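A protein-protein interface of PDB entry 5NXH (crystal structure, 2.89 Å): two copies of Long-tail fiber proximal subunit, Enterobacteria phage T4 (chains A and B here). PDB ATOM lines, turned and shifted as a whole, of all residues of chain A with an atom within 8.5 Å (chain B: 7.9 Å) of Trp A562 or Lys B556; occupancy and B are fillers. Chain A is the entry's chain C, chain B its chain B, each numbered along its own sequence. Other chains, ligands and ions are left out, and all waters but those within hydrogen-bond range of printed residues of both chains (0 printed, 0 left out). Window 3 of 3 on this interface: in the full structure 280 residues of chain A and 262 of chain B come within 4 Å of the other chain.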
ATOM      1  N   ARG A 543      -5.338  15.854  21.793  1.00  0.00           N
ATOM      2  CA  ARG A 543      -5.092  17.274  22.008  1.00  0.00           C
ATOM      3  C   ARG A 543      -6.333  18.082  21.652  1.00  0.00           C
ATOM      4  O   ARG A 543      -6.922  17.885  20.593  1.00  0.00           O
ATOM      5  CB  ARG A 543      -3.905  17.706  21.171  1.00  0.00           C
ATOM      6  CG  ARG A 543      -3.522  19.127  21.394  1.00  0.00           C
ATOM      7  CD  ARG A 543      -2.139  19.449  20.848  1.00  0.00           C
ATOM      8  NE  ARG A 543      -1.976  20.902  20.788  1.00  0.00           N
ATOM      9  CZ  ARG A 543      -0.914  21.555  20.337  1.00  0.00           C
ATOM     10  NH1 ARG A 543       0.159  20.891  19.909  1.00  0.00           N
ATOM     11  NH2 ARG A 543      -0.927  22.896  20.341  1.00  0.00           N
ATOM     12  N   ILE A 544      -6.742  18.983  22.533  1.00  0.00           N
ATOM     13  CA  ILE A 544      -7.821  19.933  22.219  1.00  0.00           C
ATOM     14  C   ILE A 544      -7.316  21.363  22.397  1.00  0.00           C
ATOM     15  O   ILE A 544      -7.085  21.814  23.520  1.00  0.00           O
ATOM     16  CB  ILE A 544      -9.074  19.720  23.079  1.00  0.00           C
ATOM     17  CG1 ILE A 544      -9.472  18.251  23.040  1.00  0.00           C
ATOM     18  CG2 ILE A 544     -10.227  20.598  22.569  1.00  0.00           C
ATOM     19  CD1 ILE A 544     -10.842  17.982  23.617  1.00  0.00           C
ATOM     20  N   GLY A 545      -7.162  22.080  21.288  1.00  0.00           N
ATOM     21  CA  GLY A 545      -6.454  23.348  21.316  1.00  0.00           C
ATOM     22  C   GLY A 545      -5.036  23.098  21.798  1.00  0.00           C
ATOM     23  O   GLY A 545      -4.339  22.265  21.230  1.00  0.00           O
ATOM     24  N   ASN A 546      -4.621  23.796  22.853  1.00  0.00           N
ATOM     25  CA  ASN A 546      -3.279  23.620  23.419  1.00  0.00           C
ATOM     26  C   ASN A 546      -3.261  22.698  24.648  1.00  0.00           C
ATOM     27  O   ASN A 546      -2.209  22.563  25.279  1.00  0.00           O
ATOM     28  CB  ASN A 546      -2.653  24.977  23.764  1.00  0.00           C
ATOM     29  CG  ASN A 546      -2.468  25.871  22.545  1.00  0.00           C
ATOM     30  OD1 ASN A 546      -2.037  25.424  21.465  1.00  0.00           O
ATOM     31  ND2 ASN A 546      -2.815  27.153  22.721  1.00  0.00           N
ATOM     32  N   VAL A 547      -4.401  22.083  24.996  1.00  0.00           N
ATOM     33  CA  VAL A 547      -4.432  21.072  26.058  1.00  0.00           C
ATOM     34  C   VAL A 547      -4.342  19.651  25.508  1.00  0.00           C
ATOM     35  O   VAL A 547      -4.978  19.318  24.519  1.00  0.00           O
ATOM     36  CB  VAL A 547      -5.666  21.201  26.980  1.00  0.00           C
ATOM     37  CG1 VAL A 547      -6.937  20.590  26.405  1.00  0.00           C
ATOM     38  CG2 VAL A 547      -5.358  20.549  28.334  1.00  0.00           C
ATOM     39  N   ARG A 548      -3.566  18.829  26.194  1.00  0.00           N
ATOM     40  CA  ARG A 548      -3.263  17.466  25.783  1.00  0.00           C
ATOM     41  C   ARG A 548      -3.836  16.511  26.825  1.00  0.00           C
ATOM     42  O   ARG A 548      -3.346  16.456  27.945  1.00  0.00           O
ATOM     43  CB  ARG A 548      -1.741  17.317  25.671  1.00  0.00           C
ATOM     44  CG  ARG A 548      -1.295  16.131  24.860  1.00  0.00           C
ATOM     45  CD  ARG A 548       0.194  16.170  24.590  1.00  0.00           C
ATOM     46  NE  ARG A 548       0.712  14.803  24.604  1.00  0.00           N
ATOM     47  CZ  ARG A 548       1.795  14.378  23.958  1.00  0.00           C
ATOM     48  NH1 ARG A 548       2.533  15.203  23.219  1.00  0.00           N
ATOM     49  NH2 ARG A 548       2.157  13.101  24.072  1.00  0.00           N
ATOM     50  N   ILE A 549      -4.890  15.785  26.468  1.00  0.00           N
ATOM     51  CA  ILE A 549      -5.521  14.825  27.385  1.00  0.00           C
ATOM     52  C   ILE A 549      -4.887  13.437  27.181  1.00  0.00           C
ATOM     53  O   ILE A 549      -5.044  12.824  26.119  1.00  0.00           O
ATOM     54  CB  ILE A 549      -7.053  14.768  27.176  1.00  0.00           C
ATOM     55  CG1 ILE A 549      -7.673  16.166  27.185  1.00  0.00           C
ATOM     56  CG2 ILE A 549      -7.693  13.943  28.270  1.00  0.00           C
ATOM     57  CD1 ILE A 549      -9.137  16.168  26.821  1.00  0.00           C
ATOM     58  N   LYS A 559      -4.554  12.782  32.706  1.00  0.00           N
ATOM     59  CA  LYS A 559      -3.866  14.052  32.977  1.00  0.00           C
ATOM     60  C   LYS A 559      -4.276  15.072  31.933  1.00  0.00           C
ATOM     61  O   LYS A 559      -4.658  14.710  30.821  1.00  0.00           O
ATOM     62  CB  LYS A 559      -2.342  13.913  32.930  1.00  0.00           C
ATOM     63  CG  LYS A 559      -1.802  12.746  33.727  1.00  0.00           C
ATOM     64  CD  LYS A 559      -0.283  12.750  33.814  1.00  0.00           C
ATOM     65  CE  LYS A 559       0.202  11.471  34.488  1.00  0.00           C
ATOM     66  NZ  LYS A 559       1.614  11.131  34.152  1.00  0.00           N
ATOM     67  N   PHE A 560      -4.226  16.344  32.335  1.00  0.00           N
ATOM     68  CA  PHE A 560      -4.376  17.493  31.439  1.00  0.00           C
ATOM     69  C   PHE A 560      -3.004  18.202  31.429  1.00  0.00           C
ATOM     70  O   PHE A 560      -2.575  18.749  32.457  1.00  0.00           O
ATOM     71  CB  PHE A 560      -5.434  18.480  31.952  1.00  0.00           C
ATOM     72  CG  PHE A 560      -6.867  18.005  31.846  1.00  0.00           C
ATOM     73  CD1 PHE A 560      -7.261  16.709  32.154  1.00  0.00           C
ATOM     74  CD2 PHE A 560      -7.870  18.923  31.496  1.00  0.00           C
ATOM     75  CE1 PHE A 560      -8.597  16.327  32.086  1.00  0.00           C
ATOM     76  CE2 PHE A 560      -9.204  18.534  31.413  1.00  0.00           C
ATOM     77  CZ  PHE A 560      -9.568  17.237  31.713  1.00  0.00           C
ATOM     78  N   GLU A 561      -2.315  18.191  30.288  1.00  0.00           N
ATOM     79  CA  GLU A 561      -1.071  18.950  30.115  1.00  0.00           C
ATOM     80  C   GLU A 561      -1.326  20.137  29.176  1.00  0.00           C
ATOM     81  O   GLU A 561      -1.901  19.949  28.111  1.00  0.00           O
ATOM     82  CB  GLU A 561       0.007  18.068  29.490  1.00  0.00           C
ATOM     83  CG  GLU A 561       0.303  16.765  30.225  1.00  0.00           C
ATOM     84  CD  GLU A 561       1.159  15.798  29.412  1.00  0.00           C
ATOM     85  OE1 GLU A 561       1.469  16.087  28.224  1.00  0.00           O
ATOM     86  OE2 GLU A 561       1.524  14.742  29.981  1.00  0.00           O
ATOM     87  N   TRP A 562      -0.893  21.344  29.554  1.00  0.00           N
ATOM     88  CA  TRP A 562      -0.914  22.495  28.639  1.00  0.00           C
ATOM     89  C   TRP A 562       0.404  22.518  27.859  1.00  0.00           C
ATOM     90  O   TRP A 562       1.458  22.492  28.460  1.00  0.00           O
ATOM     91  CB  TRP A 562      -1.111  23.794  29.409  1.00  0.00           C
ATOM     92  CG  TRP A 562      -1.093  25.001  28.529  1.00  0.00           C
ATOM     93  CD1 TRP A 562      -0.001  25.746  28.182  1.00  0.00           C
ATOM     94  CD2 TRP A 562      -2.214  25.610  27.881  1.00  0.00           C
ATOM     95  NE1 TRP A 562      -0.364  26.774  27.354  1.00  0.00           N
ATOM     96  CE2 TRP A 562      -1.717  26.721  27.152  1.00  0.00           C
ATOM     97  CE3 TRP A 562      -3.585  25.328  27.842  1.00  0.00           C
ATOM     98  CZ2 TRP A 562      -2.548  27.555  26.385  1.00  0.00           C
ATOM     99  CZ3 TRP A 562      -4.411  26.140  27.055  1.00  0.00           C
ATOM    100  CH2 TRP A 562      -3.882  27.247  26.336  1.00  0.00           C
ATOM    101  N   VAL A 563       0.349  22.594  26.532  1.00  0.00           N
ATOM    102  CA  VAL A 563       1.545  22.300  25.725  1.00  0.00           C
ATOM    103  C   VAL A 563       2.317  23.529  25.268  1.00  0.00           C
ATOM    104  O   VAL A 563       3.522  23.536  25.447  1.00  0.00           O
ATOM    105  CB  VAL A 563       1.283  21.350  24.545  1.00  0.00           C
ATOM    106  CG1 VAL A 563       0.526  20.110  25.010  1.00  0.00           C
ATOM    107  CG2 VAL A 563       0.523  22.026  23.428  1.00  0.00           C
ATOM    108  N   GLU A 564       1.658  24.540  24.700  1.00  0.00           N
ATOM    109  CA  GLU A 564       2.389  25.592  23.958  1.00  0.00           C
ATOM    110  C   GLU A 564       2.955  26.639  24.919  1.00  0.00           C
ATOM    111  O   GLU A 564       3.604  27.606  24.481  1.00  0.00           O
ATOM    112  CB  GLU A 564       1.502  26.246  22.877  1.00  0.00           C
ATOM    113  CG  GLU A 564       2.267  26.763  21.669  1.00  0.00           C
ATOM    114  CD  GLU A 564       1.549  27.896  20.952  1.00  0.00           C
ATOM    115  OE1 GLU A 564       0.292  27.991  21.001  1.00  0.00           O
ATOM    116  OE2 GLU A 564       2.267  28.710  20.341  1.00  0.00           O
ATOM    117  OXT GLU A 564       2.797  26.602  26.148  1.00  0.00           O
ATOM    118  N   PRO B 551     -10.990  24.853  24.501  1.00  0.00           N
ATOM    119  CA  PRO B 551      -9.839  25.339  25.262  1.00  0.00           C
ATOM    120  C   PRO B 551     -10.102  26.647  26.027  1.00  0.00           C
ATOM    121  O   PRO B 551     -10.754  27.553  25.503  1.00  0.00           O
ATOM    122  CB  PRO B 551      -8.776  25.556  24.183  1.00  0.00           C
ATOM    123  CG  PRO B 551      -9.558  25.807  22.930  1.00  0.00           C
ATOM    124  CD  PRO B 551     -10.712  24.855  23.045  1.00  0.00           C
ATOM    125  N   ASP B 552      -9.586  26.711  27.261  1.00  0.00           N
ATOM    126  CA  ASP B 552      -9.570  27.917  28.100  1.00  0.00           C
ATOM    127  C   ASP B 552      -8.105  28.382  28.275  1.00  0.00           C
ATOM    128  O   ASP B 552      -7.402  27.874  29.166  1.00  0.00           O
ATOM    129  CB  ASP B 552     -10.188  27.592  29.464  1.00  0.00           C
ATOM    130  CG  ASP B 552     -10.357  28.815  30.366  1.00  0.00           C
ATOM    131  OD1 ASP B 552     -10.370  29.969  29.871  1.00  0.00           O
ATOM    132  OD2 ASP B 552     -10.493  28.603  31.589  1.00  0.00           O
ATOM    133  N   PRO B 553      -7.638  29.343  27.430  1.00  0.00           N
ATOM    134  CA  PRO B 553      -6.235  29.766  27.536  1.00  0.00           C
ATOM    135  C   PRO B 553      -5.881  30.494  28.841  1.00  0.00           C
ATOM    136  O   PRO B 553      -4.711  30.495  29.250  1.00  0.00           O
ATOM    137  CB  PRO B 553      -6.055  30.692  26.320  1.00  0.00           C
ATOM    138  CG  PRO B 553      -7.421  31.233  26.071  1.00  0.00           C
ATOM    139  CD  PRO B 553      -8.354  30.110  26.391  1.00  0.00           C
ATOM    140  N   VAL B 554      -6.887  31.073  29.497  1.00  0.00           N
ATOM    141  CA  VAL B 554      -6.663  31.971  30.633  1.00  0.00           C
ATOM    142  C   VAL B 554      -6.409  31.191  31.940  1.00  0.00           C
ATOM    143  O   VAL B 554      -5.593  31.628  32.746  1.00  0.00           O
ATOM    144  CB  VAL B 554      -7.813  33.000  30.802  1.00  0.00           C
ATOM    145  CG1 VAL B 554      -7.349  34.152  31.698  1.00  0.00           C
ATOM    146  CG2 VAL B 554      -8.280  33.545  29.441  1.00  0.00           C
ATOM    147  N   ASN B 555      -7.094  30.062  32.149  1.00  0.00           N
ATOM    148  CA  ASN B 555      -6.819  29.171  33.306  1.00  0.00           C
ATOM    149  C   ASN B 555      -5.865  28.024  33.001  1.00  0.00           C
ATOM    150  O   ASN B 555      -5.528  27.256  33.908  1.00  0.00           O
ATOM    151  CB  ASN B 555      -8.105  28.561  33.863  1.00  0.00           C
ATOM    152  CG  ASN B 555      -9.083  29.602  34.322  1.00  0.00           C
ATOM    153  OD1 ASN B 555      -9.380  30.547  33.589  1.00  0.00           O
ATOM    154  ND2 ASN B 555      -9.596  29.441  35.540  1.00  0.00           N
ATOM    155  N   LYS B 556      -5.454  27.896  31.736  1.00  0.00           N
ATOM    156  CA  LYS B 556      -4.588  26.796  31.275  1.00  0.00           C
ATOM    157  C   LYS B 556      -5.203  25.402  31.487  1.00  0.00           C
ATOM    158  O   LYS B 556      -4.554  24.462  31.965  1.00  0.00           O
ATOM    159  CB  LYS B 556      -3.160  26.934  31.858  1.00  0.00           C
ATOM    160  CG  LYS B 556      -2.580  28.350  31.677  1.00  0.00           C
ATOM    161  CD  LYS B 556      -1.146  28.471  31.147  1.00  0.00           C
ATOM    162  CE  LYS B 556      -1.018  29.759  30.339  1.00  0.00           C
ATOM    163  NZ  LYS B 556       0.331  29.890  29.739  1.00  0.00           N
ATOM    164  N   THR B 557      -6.478  25.306  31.094  1.00  0.00           N
ATOM    165  CA  THR B 557      -7.257  24.055  31.098  1.00  0.00           C
ATOM    166  C   THR B 557      -8.404  24.161  30.052  1.00  0.00           C
ATOM    167  O   THR B 557      -8.218  24.803  29.015  1.00  0.00           O
ATOM    168  CB  THR B 557      -7.748  23.687  32.530  1.00  0.00           C
ATOM    169  OG1 THR B 557      -8.435  22.423  32.511  1.00  0.00           O
ATOM    170  CG2 THR B 557      -8.676  24.777  33.118  1.00  0.00           C
ATOM    171  N   VAL B 558      -9.542  23.513  30.292  1.00  0.00           N
ATOM    172  CA  VAL B 558     -10.598  23.391  29.278  1.00  0.00           C
ATOM    173  C   VAL B 558     -11.972  23.622  29.908  1.00  0.00           C
ATOM    174  O   VAL B 558     -12.191  23.205  31.032  1.00  0.00           O
ATOM    175  CB  VAL B 558     -10.528  21.981  28.629  1.00  0.00           C
ATOM    176  CG1 VAL B 558     -11.007  20.877  29.579  1.00  0.00           C
ATOM    177  CG2 VAL B 558     -11.223  21.897  27.300  1.00  0.00           C
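The backbone carbonyl oxygen (O) of Thr B557 lies within hydrogen-bond range of the backbone NH (N) of Asp B552 (2.9 Å).
The indole nitrogen of Trp A562 sits at hydrogen-bond distance from the chain-end carboxylate of Glu A564, 3.4 Å away.
Among the printed residues, pairs that only touch across the chains: Phe A560 with Val B558, Trp A562 with Pro B553, Phe A560 with Thr B557 and Trp A562 with Lys B556.
Trp A562 touches just these residues of chain B: Pro B553 (3.6 Å) and Lys B556 (3.9 Å).
Lys B556 touches just one residue of chain A: Trp A562 (3.9 Å).
Thr B557 touches one residue of chain A.
Printed residues of chain B within 4 Å of Phe A560: Thr B557 (3.7 Å) and Val B558 (3.5 Å).
Of the printed residues of chain A, Pro B553 touches Trp A562.
Printed residues of chain A within 4 Å of Val B558: Phe A560.
Pro B551 touches none of the printed residues of chain A.
Arg A543 touches none of the printed residues of chain B.
The nearest residue of chain B that does not touch Trp A562 is Asp B552 (4.1 Å).
The nearest residue of chain A that does not touch Lys B556 is Val A547 (5.4 Å).
Of the 8 printed residues of chain B, 4 touch a printed residue of chain A.
Hydrophobic or aromatic side chains of chain A that line the printed part of chain B: Phe A560 and Trp A562.
Among the printed residues, no Asp or Glu carboxylate lies within 4 Å of a Lys or Arg side-chain nitrogen of the other chain.
No position is printed for both chains.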
